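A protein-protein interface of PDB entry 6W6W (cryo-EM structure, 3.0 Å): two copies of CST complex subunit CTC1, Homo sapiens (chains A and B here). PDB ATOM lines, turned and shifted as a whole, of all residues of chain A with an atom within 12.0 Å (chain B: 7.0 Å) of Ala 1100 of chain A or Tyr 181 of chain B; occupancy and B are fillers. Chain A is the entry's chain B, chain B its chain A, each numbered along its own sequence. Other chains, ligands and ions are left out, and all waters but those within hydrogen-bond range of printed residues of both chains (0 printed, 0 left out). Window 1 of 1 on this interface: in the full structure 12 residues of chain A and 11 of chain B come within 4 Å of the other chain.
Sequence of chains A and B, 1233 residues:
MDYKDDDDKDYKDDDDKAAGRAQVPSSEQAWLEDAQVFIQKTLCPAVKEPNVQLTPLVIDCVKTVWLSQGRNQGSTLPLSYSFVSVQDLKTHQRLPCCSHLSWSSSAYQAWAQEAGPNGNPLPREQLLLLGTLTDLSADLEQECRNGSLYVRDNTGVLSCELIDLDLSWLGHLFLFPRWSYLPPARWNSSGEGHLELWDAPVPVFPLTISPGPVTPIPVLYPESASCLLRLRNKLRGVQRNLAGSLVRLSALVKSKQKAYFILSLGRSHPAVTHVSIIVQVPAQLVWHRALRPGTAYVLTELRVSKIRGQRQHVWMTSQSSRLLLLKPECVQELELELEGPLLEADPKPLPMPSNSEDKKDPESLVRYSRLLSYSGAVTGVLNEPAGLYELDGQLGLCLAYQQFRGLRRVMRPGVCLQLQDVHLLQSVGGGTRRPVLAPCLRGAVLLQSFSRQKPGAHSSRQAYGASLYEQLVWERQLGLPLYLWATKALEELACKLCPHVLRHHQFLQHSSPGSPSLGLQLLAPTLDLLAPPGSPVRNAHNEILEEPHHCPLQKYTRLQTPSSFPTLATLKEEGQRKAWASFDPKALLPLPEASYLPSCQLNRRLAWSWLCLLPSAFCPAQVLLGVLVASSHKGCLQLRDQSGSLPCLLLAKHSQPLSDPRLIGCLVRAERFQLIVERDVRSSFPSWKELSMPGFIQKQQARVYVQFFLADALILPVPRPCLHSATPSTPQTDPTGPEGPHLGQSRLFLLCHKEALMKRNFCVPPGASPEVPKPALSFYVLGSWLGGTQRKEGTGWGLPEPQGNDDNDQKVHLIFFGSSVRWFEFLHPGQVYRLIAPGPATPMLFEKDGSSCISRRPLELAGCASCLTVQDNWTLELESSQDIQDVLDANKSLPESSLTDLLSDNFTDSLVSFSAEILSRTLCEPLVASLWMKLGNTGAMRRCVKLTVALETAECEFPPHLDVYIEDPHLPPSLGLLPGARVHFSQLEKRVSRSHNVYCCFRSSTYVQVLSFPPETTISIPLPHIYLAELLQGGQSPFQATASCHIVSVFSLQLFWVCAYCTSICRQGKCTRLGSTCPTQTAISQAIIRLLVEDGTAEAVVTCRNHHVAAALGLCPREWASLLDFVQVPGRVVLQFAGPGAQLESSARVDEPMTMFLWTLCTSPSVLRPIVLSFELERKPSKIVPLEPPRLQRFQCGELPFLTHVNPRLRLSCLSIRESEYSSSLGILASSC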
ATOM      1  N   ALA A1087       2.713   0.571  -0.807  1.00  0.00           N
ATOM      2  CA  ALA A1087       3.222   0.477   0.561  1.00  0.00           C
ATOM      3  C   ALA A1087       2.099   0.295   1.575  1.00  0.00           C
ATOM      4  O   ALA A1087       1.106   1.025   1.563  1.00  0.00           O
ATOM      5  CB  ALA A1087       4.029   1.728   0.902  1.00  0.00           C
ATOM      6  N   ILE A1088       2.267  -0.690   2.454  1.00  0.00           N
ATOM      7  CA  ILE A1088       1.241  -1.092   3.399  1.00  0.00           C
ATOM      8  C   ILE A1088       1.546  -0.535   4.787  1.00  0.00           C
ATOM      9  O   ILE A1088       2.558   0.130   5.015  1.00  0.00           O
ATOM     10  CB  ILE A1088       1.117  -2.616   3.435  1.00  0.00           C
ATOM     11  N   ILE A1089       0.644  -0.820   5.731  1.00  0.00           N
ATOM     12  CA  ILE A1089       0.816  -0.353   7.101  1.00  0.00           C
ATOM     13  C   ILE A1089       1.916  -1.103   7.837  1.00  0.00           C
ATOM     14  O   ILE A1089       2.435  -0.594   8.835  1.00  0.00           O
ATOM     15  CB  ILE A1089      -0.499  -0.480   7.867  1.00  0.00           C
ATOM     16  N   ARG A1090       2.280  -2.299   7.373  1.00  0.00           N
ATOM     17  CA  ARG A1090       3.388  -3.037   7.962  1.00  0.00           C
ATOM     18  C   ARG A1090       4.729  -2.647   7.362  1.00  0.00           C
ATOM     19  O   ARG A1090       5.761  -2.792   8.026  1.00  0.00           O
ATOM     20  CB  ARG A1090       3.168  -4.543   7.794  1.00  0.00           C
ATOM     21  N   LEU A1091       4.739  -2.153   6.125  1.00  0.00           N
ATOM     22  CA  LEU A1091       5.985  -1.715   5.511  1.00  0.00           C
ATOM     23  C   LEU A1091       6.434  -0.365   6.044  1.00  0.00           C
ATOM     24  O   LEU A1091       7.635  -0.074   6.048  1.00  0.00           O
ATOM     25  CB  LEU A1091       5.834  -1.654   3.991  1.00  0.00           C
ATOM     26  N   LEU A1092       5.496   0.470   6.490  1.00  0.00           N
ATOM     27  CA  LEU A1092       5.857   1.739   7.104  1.00  0.00           C
ATOM     28  C   LEU A1092       6.221   1.584   8.571  1.00  0.00           C
ATOM     29  O   LEU A1092       6.859   2.477   9.135  1.00  0.00           O
ATOM     30  CB  LEU A1092       4.715   2.747   6.955  1.00  0.00           C
ATOM     31  N   VAL A1093       5.828   0.480   9.200  1.00  0.00           N
ATOM     32  CA  VAL A1093       6.203   0.203  10.577  1.00  0.00           C
ATOM     33  C   VAL A1093       7.491  -0.600  10.687  1.00  0.00           C
ATOM     34  O   VAL A1093       8.058  -0.684  11.782  1.00  0.00           O
ATOM     35  CB  VAL A1093       5.073  -0.541  11.295  1.00  0.00           C
ATOM     36  N   GLU A1094       7.964  -1.185   9.588  1.00  0.00           N
ATOM     37  CA  GLU A1094       9.227  -1.908   9.559  1.00  0.00           C
ATOM     38  C   GLU A1094      10.298  -1.196   8.745  1.00  0.00           C
ATOM     39  O   GLU A1094      11.397  -1.735   8.591  1.00  0.00           O
ATOM     40  CB  GLU A1094       9.016  -3.322   9.006  1.00  0.00           C
ATOM     41  N   ASP A1095      10.008  -0.008   8.225  1.00  0.00           N
ATOM     42  CA  ASP A1095      10.972   0.780   7.470  1.00  0.00           C
ATOM     43  C   ASP A1095      10.573   2.247   7.573  1.00  0.00           C
ATOM     44  O   ASP A1095       9.554   2.585   8.180  1.00  0.00           O
ATOM     45  CB  ASP A1095      11.046   0.320   6.011  1.00  0.00           C
ATOM     46  N   GLY A1096      11.397   3.110   6.960  1.00  0.00           N
ATOM     47  CA  GLY A1096      11.210   4.569   6.920  1.00  0.00           C
ATOM     48  C   GLY A1096      11.079   5.168   8.318  1.00  0.00           C
ATOM     49  O   GLY A1096      10.247   6.043   8.562  1.00  0.00           O
ATOM     50  N   THR A1097      11.911   4.695   9.244  1.00  0.00           N
ATOM     51  CA  THR A1097      11.833   5.107  10.645  1.00  0.00           C
ATOM     52  C   THR A1097      12.697   6.342  10.900  1.00  0.00           C
ATOM     53  O   THR A1097      13.596   6.352  11.739  1.00  0.00           O
ATOM     54  CB  THR A1097      12.233   3.952  11.554  1.00  0.00           C
ATOM     55  N   ALA A1098      12.403   7.405  10.147  1.00  0.00           N
ATOM     56  CA  ALA A1098      13.075   8.684  10.329  1.00  0.00           C
ATOM     57  C   ALA A1098      12.097   9.848  10.220  1.00  0.00           C
ATOM     58  O   ALA A1098      12.479  10.938   9.776  1.00  0.00           O
ATOM     59  CB  ALA A1098      14.214   8.856   9.323  1.00  0.00           C
ATOM     60  N   GLU A1099      10.837   9.620  10.613  1.00  0.00           N
ATOM     61  CA  GLU A1099       9.769  10.622  10.701  1.00  0.00           C
ATOM     62  C   GLU A1099       9.499  11.292   9.350  1.00  0.00           C
ATOM     63  O   GLU A1099       9.662  12.495   9.177  1.00  0.00           O
ATOM     64  CB  GLU A1099      10.077  11.661  11.788  1.00  0.00           C
ATOM     65  N   ALA A1100       9.052  10.473   8.401  1.00  0.00           N
ATOM     66  CA  ALA A1100       8.805  10.922   7.039  1.00  0.00           C
ATOM     67  C   ALA A1100       7.509  11.729   6.943  1.00  0.00           C
ATOM     68  O   ALA A1100       6.767  11.890   7.914  1.00  0.00           O
ATOM     69  CB  ALA A1100       8.753   9.724   6.094  1.00  0.00           C
ATOM     70  N   VAL A1101       7.239  12.243   5.744  1.00  0.00           N
ATOM     71  CA  VAL A1101       5.983  12.905   5.412  1.00  0.00           C
ATOM     72  C   VAL A1101       5.795  12.804   3.906  1.00  0.00           C
ATOM     73  O   VAL A1101       6.718  12.438   3.177  1.00  0.00           O
ATOM     74  CB  VAL A1101       5.963  14.365   5.869  1.00  0.00           C
ATOM     75  N   VAL A1102       4.594  13.137   3.442  1.00  0.00           N
ATOM     76  CA  VAL A1102       4.299  13.006   2.020  1.00  0.00           C
ATOM     77  C   VAL A1102       3.165  13.941   1.635  1.00  0.00           C
ATOM     78  O   VAL A1102       2.320  14.290   2.460  1.00  0.00           O
ATOM     79  CB  VAL A1102       3.934  11.565   1.647  1.00  0.00           C
ATOM     80  N   THR A1103       3.168  14.347   0.364  1.00  0.00           N
ATOM     81  CA  THR A1103       2.107  15.193  -0.178  1.00  0.00           C
ATOM     82  C   THR A1103       2.075  14.955  -1.687  1.00  0.00           C
ATOM     83  O   THR A1103       2.917  15.491  -2.412  1.00  0.00           O
ATOM     84  CB  THR A1103       2.343  16.658   0.153  1.00  0.00           C
ATOM     85  N   CYS A1104       1.105  14.169  -2.147  1.00  0.00           N
ATOM     86  CA  CYS A1104       1.017  13.801  -3.556  1.00  0.00           C
ATOM     87  C   CYS A1104       0.312  14.847  -4.414  1.00  0.00           C
ATOM     88  O   CYS A1104      -0.027  14.547  -5.563  1.00  0.00           O
ATOM     89  CB  CYS A1104       0.307  12.455  -3.708  1.00  0.00           C
ATOM     90  N   LEU A1115       8.938  25.540   9.620  1.00  0.00           N
ATOM     91  CA  LEU A1115       8.995  24.086   9.526  1.00  0.00           C
ATOM     92  C   LEU A1115      10.462  23.703   9.410  1.00  0.00           C
ATOM     93  O   LEU A1115      11.342  24.567   9.429  1.00  0.00           O
ATOM     94  CB  LEU A1115       8.200  23.559   8.329  1.00  0.00           C
ATOM     95  N   CYS A1116      10.735  22.400   9.303  1.00  0.00           N
ATOM     96  CA  CYS A1116      12.053  22.069   8.787  1.00  0.00           C
ATOM     97  C   CYS A1116      11.968  21.323   7.463  1.00  0.00           C
ATOM     98  O   CYS A1116      12.099  21.962   6.413  1.00  0.00           O
ATOM     99  CB  CYS A1116      12.822  21.240   9.815  1.00  0.00           C
ATOM    100  N   PRO A1117      11.632  20.020   7.512  1.00  0.00           N
ATOM    101  CA  PRO A1117      11.362  19.116   6.385  1.00  0.00           C
ATOM    102  C   PRO A1117      11.160  17.690   6.880  1.00  0.00           C
ATOM    103  O   PRO A1117      11.576  17.373   7.998  1.00  0.00           O
ATOM    104  CB  PRO A1117      12.501  19.066   5.351  1.00  0.00           C
ATOM    105  N   ARG A1118      10.479  16.852   6.080  1.00  0.00           N
ATOM    106  CA  ARG A1118      10.938  15.491   5.761  1.00  0.00           C
ATOM    107  C   ARG A1118      10.146  15.038   4.534  1.00  0.00           C
ATOM    108  O   ARG A1118       8.998  14.615   4.674  1.00  0.00           O
ATOM    109  CB  ARG A1118      10.755  14.517   6.909  1.00  0.00           C
ATOM    110  N   GLU A1119      10.754  15.099   3.358  1.00  0.00           N
ATOM    111  CA  GLU A1119      10.013  14.777   2.146  1.00  0.00           C
ATOM    112  C   GLU A1119      10.168  13.307   1.779  1.00  0.00           C
ATOM    113  O   GLU A1119      11.193  12.681   2.059  1.00  0.00           O
ATOM    114  CB  GLU A1119      10.469  15.655   0.981  1.00  0.00           C
ATOM    115  N   TRP A1120       9.133  12.762   1.145  1.00  0.00           N
ATOM    116  CA  TRP A1120       9.149  11.401   0.621  1.00  0.00           C
ATOM    117  C   TRP A1120       8.106  11.314  -0.484  1.00  0.00           C
ATOM    118  O   TRP A1120       7.377  12.273  -0.750  1.00  0.00           O
ATOM    119  CB  TRP A1120       8.887  10.365   1.716  1.00  0.00           C
ATOM    120  N   ALA A1121       8.034  10.152  -1.130  1.00  0.00           N
ATOM    121  CA  ALA A1121       7.134   9.968  -2.263  1.00  0.00           C
ATOM    122  C   ALA A1121       6.441   8.615  -2.199  1.00  0.00           C
ATOM    123  O   ALA A1121       6.273   7.938  -3.218  1.00  0.00           O
ATOM    124  CB  ALA A1121       7.878  10.124  -3.589  1.00  0.00           C
ATOM    125  N   SER A1122       6.024   8.202  -1.006  1.00  0.00           N
ATOM    126  CA  SER A1122       5.266   6.969  -0.874  1.00  0.00           C
ATOM    127  C   SER A1122       3.780   7.233  -1.107  1.00  0.00           C
ATOM    128  O   SER A1122       3.330   8.376  -1.197  1.00  0.00           O
ATOM    129  CB  SER A1122       5.493   6.343   0.500  1.00  0.00           C
ATOM    130  N   LEU A1123       3.009   6.152  -1.206  1.00  0.00           N
ATOM    131  CA  LEU A1123       1.574   6.249  -1.476  1.00  0.00           C
ATOM    132  C   LEU A1123       0.851   5.225  -0.607  1.00  0.00           C
ATOM    133  O   LEU A1123       0.887   4.025  -0.893  1.00  0.00           O
ATOM    134  CB  LEU A1123       1.273   6.036  -2.956  1.00  0.00           C
ATOM    135  N   LEU A1124       0.192   5.702   0.446  1.00  0.00           N
ATOM    136  CA  LEU A1124      -0.564   4.849   1.352  1.00  0.00           C
ATOM    137  C   LEU A1124      -2.044   4.899   1.007  1.00  0.00           C
ATOM    138  O   LEU A1124      -2.568   5.945   0.617  1.00  0.00           O
ATOM    139  CB  LEU A1124      -0.362   5.266   2.809  1.00  0.00           C
ATOM    140  N   ASP A1125      -2.711   3.762   1.157  1.00  0.00           N
ATOM    141  CA  ASP A1125      -4.120   3.647   0.830  1.00  0.00           C
ATOM    142  C   ASP A1125      -4.750   2.522   1.631  1.00  0.00           C
ATOM    143  O   ASP A1125      -5.526   1.730   1.099  1.00  0.00           O
ATOM    144  CB  ASP A1125      -4.306   3.409  -0.661  1.00  0.00           C
ATOM    145  N   SER B 159      -3.283   1.399  12.078  1.00  0.00           N
ATOM    146  CA  SER B 159      -1.998   1.964  12.465  1.00  0.00           C
ATOM    147  C   SER B 159      -2.115   3.385  12.995  1.00  0.00           C
ATOM    148  O   SER B 159      -1.430   4.277  12.493  1.00  0.00           O
ATOM    149  CB  SER B 159      -1.030   1.949  11.288  1.00  0.00           C
ATOM    150  OG  SER B 159       0.194   2.565  11.646  1.00  0.00           O
ATOM    151  N   TRP B 179      -0.362  12.078   3.484  1.00  0.00           N
ATOM    152  CA  TRP B 179       0.333  11.235   4.449  1.00  0.00           C
ATOM    153  C   TRP B 179       1.253  12.030   5.376  1.00  0.00           C
ATOM    154  O   TRP B 179       1.744  13.104   5.026  1.00  0.00           O
ATOM    155  CB  TRP B 179       1.143  10.210   3.658  1.00  0.00           C
ATOM    156  CG  TRP B 179       1.505   8.968   4.334  1.00  0.00           C
ATOM    157  CD1 TRP B 179       0.662   7.998   4.762  1.00  0.00           C
ATOM    158  CD2 TRP B 179       2.827   8.507   4.607  1.00  0.00           C
ATOM    159  NE1 TRP B 179       1.374   6.964   5.315  1.00  0.00           N
ATOM    160  CE2 TRP B 179       2.709   7.255   5.233  1.00  0.00           C
ATOM    161  CE3 TRP B 179       4.101   9.041   4.399  1.00  0.00           C
ATOM    162  CZ2 TRP B 179       3.817   6.523   5.652  1.00  0.00           C
ATOM    163  CZ3 TRP B 179       5.200   8.315   4.815  1.00  0.00           C
ATOM    164  CH2 TRP B 179       5.052   7.069   5.432  1.00  0.00           C
ATOM    165  N   SER B 180       1.457  11.492   6.581  1.00  0.00           N
ATOM    166  CA  SER B 180       2.494  11.941   7.515  1.00  0.00           C
ATOM    167  C   SER B 180       2.666  10.854   8.562  1.00  0.00           C
ATOM    168  O   SER B 180       1.686  10.464   9.200  1.00  0.00           O
ATOM    169  CB  SER B 180       2.133  13.261   8.187  1.00  0.00           C
ATOM    170  OG  SER B 180       3.172  13.668   9.051  1.00  0.00           O
ATOM    171  N   TYR B 181       3.891  10.368   8.750  1.00  0.00           N
ATOM    172  CA  TYR B 181       4.148   9.253   9.653  1.00  0.00           C
ATOM    173  C   TYR B 181       5.216   9.636  10.664  1.00  0.00           C
ATOM    174  O   TYR B 181       6.178  10.329  10.328  1.00  0.00           O
ATOM    175  CB  TYR B 181       4.582   8.001   8.883  1.00  0.00           C
ATOM    176  CG  TYR B 181       4.929   6.816   9.756  1.00  0.00           C
ATOM    177  CD1 TYR B 181       3.936   6.017  10.301  1.00  0.00           C
ATOM    178  CD2 TYR B 181       6.253   6.489  10.024  1.00  0.00           C
ATOM    179  CE1 TYR B 181       4.250   4.933  11.097  1.00  0.00           C
ATOM    180  CE2 TYR B 181       6.575   5.411  10.822  1.00  0.00           C
ATOM    181  CZ  TYR B 181       5.570   4.639  11.353  1.00  0.00           C
ATOM    182  OH  TYR B 181       5.893   3.565  12.143  1.00  0.00           O
ATOM    183  N   LEU B 182       5.049   9.174  11.903  1.00  0.00           N
ATOM    184  CA  LEU B 182       6.029   9.406  12.951  1.00  0.00           C
ATOM    185  C   LEU B 182       6.306   8.094  13.674  1.00  0.00           C
ATOM    186  O   LEU B 182       5.362   7.403  14.085  1.00  0.00           O
ATOM    187  CB  LEU B 182       5.564  10.460  13.958  1.00  0.00           C
ATOM    188  CG  LEU B 182       5.610  11.938  13.582  1.00  0.00           C
ATOM    189  CD1 LEU B 182       4.367  12.362  12.826  1.00  0.00           C
ATOM    190  CD2 LEU B 182       5.812  12.773  14.824  1.00  0.00           C
ATOM    191  N   PRO B 183       7.570   7.731  13.868  1.00  0.00           N
ATOM    192  CA  PRO B 183       7.897   6.468  14.512  1.00  0.00           C
ATOM    193  C   PRO B 183       7.812   6.596  16.022  1.00  0.00           C
ATOM    194  O   PRO B 183       7.563   7.697  16.536  1.00  0.00           O
ATOM    195  CB  PRO B 183       9.339   6.227  14.048  1.00  0.00           C
ATOM    196  CG  PRO B 183       9.897   7.582  13.966  1.00  0.00           C
ATOM    197  CD  PRO B 183       8.781   8.485  13.519  1.00  0.00           C
ATOM    198  N   PRO B 184       7.963   5.494  16.765  1.00  0.00           N
ATOM    199  CA  PRO B 184       8.135   5.595  18.220  1.00  0.00           C
ATOM    200  C   PRO B 184       9.361   6.412  18.604  1.00  0.00           C
ATOM    201  O   PRO B 184      10.322   6.541  17.843  1.00  0.00           O
ATOM    202  CB  PRO B 184       8.289   4.138  18.657  1.00  0.00           C
ATOM    203  CG  PRO B 184       7.605   3.358  17.616  1.00  0.00           C
ATOM    204  CD  PRO B 184       7.554   4.139  16.355  1.00  0.00           C
ATOM    205  N   GLU B 192       4.336   1.384  18.352  1.00  0.00           N
ATOM    206  CA  GLU B 192       3.062   1.915  17.855  1.00  0.00           C
ATOM    207  C   GLU B 192       3.164   3.393  17.460  1.00  0.00           C
ATOM    208  O   GLU B 192       2.587   4.279  18.091  1.00  0.00           O
ATOM    209  CB  GLU B 192       1.949   1.696  18.887  1.00  0.00           C
ATOM    210  CG  GLU B 192       1.631   0.237  19.155  1.00  0.00           C
ATOM    211  CD  GLU B 192       1.016  -0.461  17.957  1.00  0.00           C
ATOM    212  OE1 GLU B 192       0.287   0.199  17.186  1.00  0.00           O
ATOM    213  OE2 GLU B 192       1.263  -1.673  17.789  1.00  0.00           O
ATOM    214  N   GLY B 193       3.939   3.637  16.405  1.00  0.00           N
ATOM    215  CA  GLY B 193       3.952   4.952  15.794  1.00  0.00           C
ATOM    216  C   GLY B 193       2.625   5.297  15.143  1.00  0.00           C
ATOM    217  O   GLY B 193       1.787   4.438  14.874  1.00  0.00           O
ATOM    218  N   HIS B 194       2.431   6.585  14.871  1.00  0.00           N
ATOM    219  CA  HIS B 194       1.121   7.091  14.494  1.00  0.00           C
ATOM    220  C   HIS B 194       1.179   7.848  13.176  1.00  0.00           C
ATOM    221  O   HIS B 194       2.247   8.182  12.663  1.00  0.00           O
ATOM    222  CB  HIS B 194       0.545   7.997  15.585  1.00  0.00           C
ATOM    223  CG  HIS B 194       1.157   9.361  15.620  1.00  0.00           C
ATOM    224  ND1 HIS B 194       2.376   9.613  16.207  1.00  0.00           N
ATOM    225  CD2 HIS B 194       0.713  10.549  15.150  1.00  0.00           C
ATOM    226  CE1 HIS B 194       2.660  10.896  16.091  1.00  0.00           C
ATOM    227  NE2 HIS B 194       1.669  11.486  15.452  1.00  0.00           N
ATOM    228  N   LEU B 195      -0.007   8.119  12.640  1.00  0.00           N
ATOM    229  CA  LEU B 195      -0.201   8.852  11.402  1.00  0.00           C
ATOM    230  C   LEU B 195      -0.794  10.223  11.694  1.00  0.00           C
ATOM    231  O   LEU B 195      -1.333  10.472  12.773  1.00  0.00           O
ATOM    232  CB  LEU B 195      -1.130   8.085  10.462  1.00  0.00           C
ATOM    233  CG  LEU B 195      -0.504   6.978   9.631  1.00  0.00           C
ATOM    234  CD1 LEU B 195      -1.571   6.003   9.189  1.00  0.00           C
ATOM    235  CD2 LEU B 195       0.191   7.577   8.439  1.00  0.00           C
ATOM    236  N   GLU B 196      -0.694  11.120  10.714  1.00  0.00           N
ATOM    237  CA  GLU B 196      -1.276  12.461  10.811  1.00  0.00           C
ATOM    238  C   GLU B 196      -1.923  12.776   9.465  1.00  0.00           C
ATOM    239  O   GLU B 196      -1.285  13.352   8.585  1.00  0.00           O
ATOM    240  CB  GLU B 196      -0.223  13.497  11.166  1.00  0.00           C
ATOM    241  CG  GLU B 196       0.296  13.463  12.586  1.00  0.00           C
ATOM    242  CD  GLU B 196       1.328  14.550  12.825  1.00  0.00           C
ATOM    243  OE1 GLU B 196       1.543  15.367  11.908  1.00  0.00           O
ATOM    244  OE2 GLU B 196       1.934  14.593  13.915  1.00  0.00           O
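The backbone NH of Tyr 181 of chain B sits at hydrogen-bond distance from the backbone carbonyl oxygen of Ala 1100 of chain A, 3.4 Å away.
The side-chain hydroxyl (OH) of Tyr 181 of chain B sits at hydrogen-bond distance from the backbone carbonyl oxygen (O) of Leu 1092 of chain A (3.3 Å).
The backbone carbonyl oxygen (O) of Trp 179 of chain B is in hydrogen-bond range of the backbone NH (N) of Val 1102 of chain A, at 3.3 Å.
Tyr 181 of chain B touches Val 1093 of chain A (OH to CA, 3.7 Å).
C of Glu 1099 of chain A touches O of Tyr 181 of chain B, 3.6 Å away.
Pro 183 of chain B touches Glu 1099 of chain A.
Leu 1124 of chain A touches Trp 179 of chain B (CB to NE1, 3.5 Å).
Of the printed residues of chain B, Ala 1100 of chain A touches Tyr 181 (2.9 Å).
Tyr 181 of chain B touches just these residues of chain A: Leu 1092, Val 1093, Glu 1099 and Ala 1100.
Of chain A, only Val 1102 and Leu 1124 come within 4 Å of Trp 179 of chain B.
No residue of chain A comes within 4 Å of Ser 180 of chain B.
No residue of chain A comes within 4 Å of Leu 182 of chain B.
Of chain A, only Glu 1099 comes within 4 Å of Pro 183 of chain B.
No residue of chain A comes within 4 Å of Pro 184 of chain B.
No residue of chain A comes within 4 Å of Gly 193 of chain B.
No residue of chain A comes within 4 Å of His 194 of chain B.
No residue of chain A comes within 4 Å of Leu 195 of chain B.
Of the printed residues of chain B, Leu 1092 of chain A touches Tyr 181 (3.3 Å).
Printed residues of chain B within 4 Å of Val 1102 of chain A: Trp 179 (2.9 Å).
Of the printed residues of chain B, Leu 1124 of chain A touches Trp 179.
Of the printed residues of chain B, Glu 1099 of chain A touches Tyr 181 and Pro 183.
Printed residues of chain B within 4 Å of Val 1093 of chain A: Tyr 181.
Thr 1097 of chain A touches none of the printed residues of chain B.
Printed residues of chain A that touch a printed residue of chain B: Leu 1092, Val 1093, Glu 1099, Ala 1100, Val 1102 and Leu 1124.
Of the 12 printed residues of chain B, 3 touch a printed residue of chain A.
Among the printed residues, no Asp or Glu carboxylate lies within 4 Å of a Lys or Arg side-chain nitrogen of the other chain.
No position is printed for both chains.
Of the 7 pairs that touch across the chains among the printed residues, none has its exchanged pair printed and touching as well.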
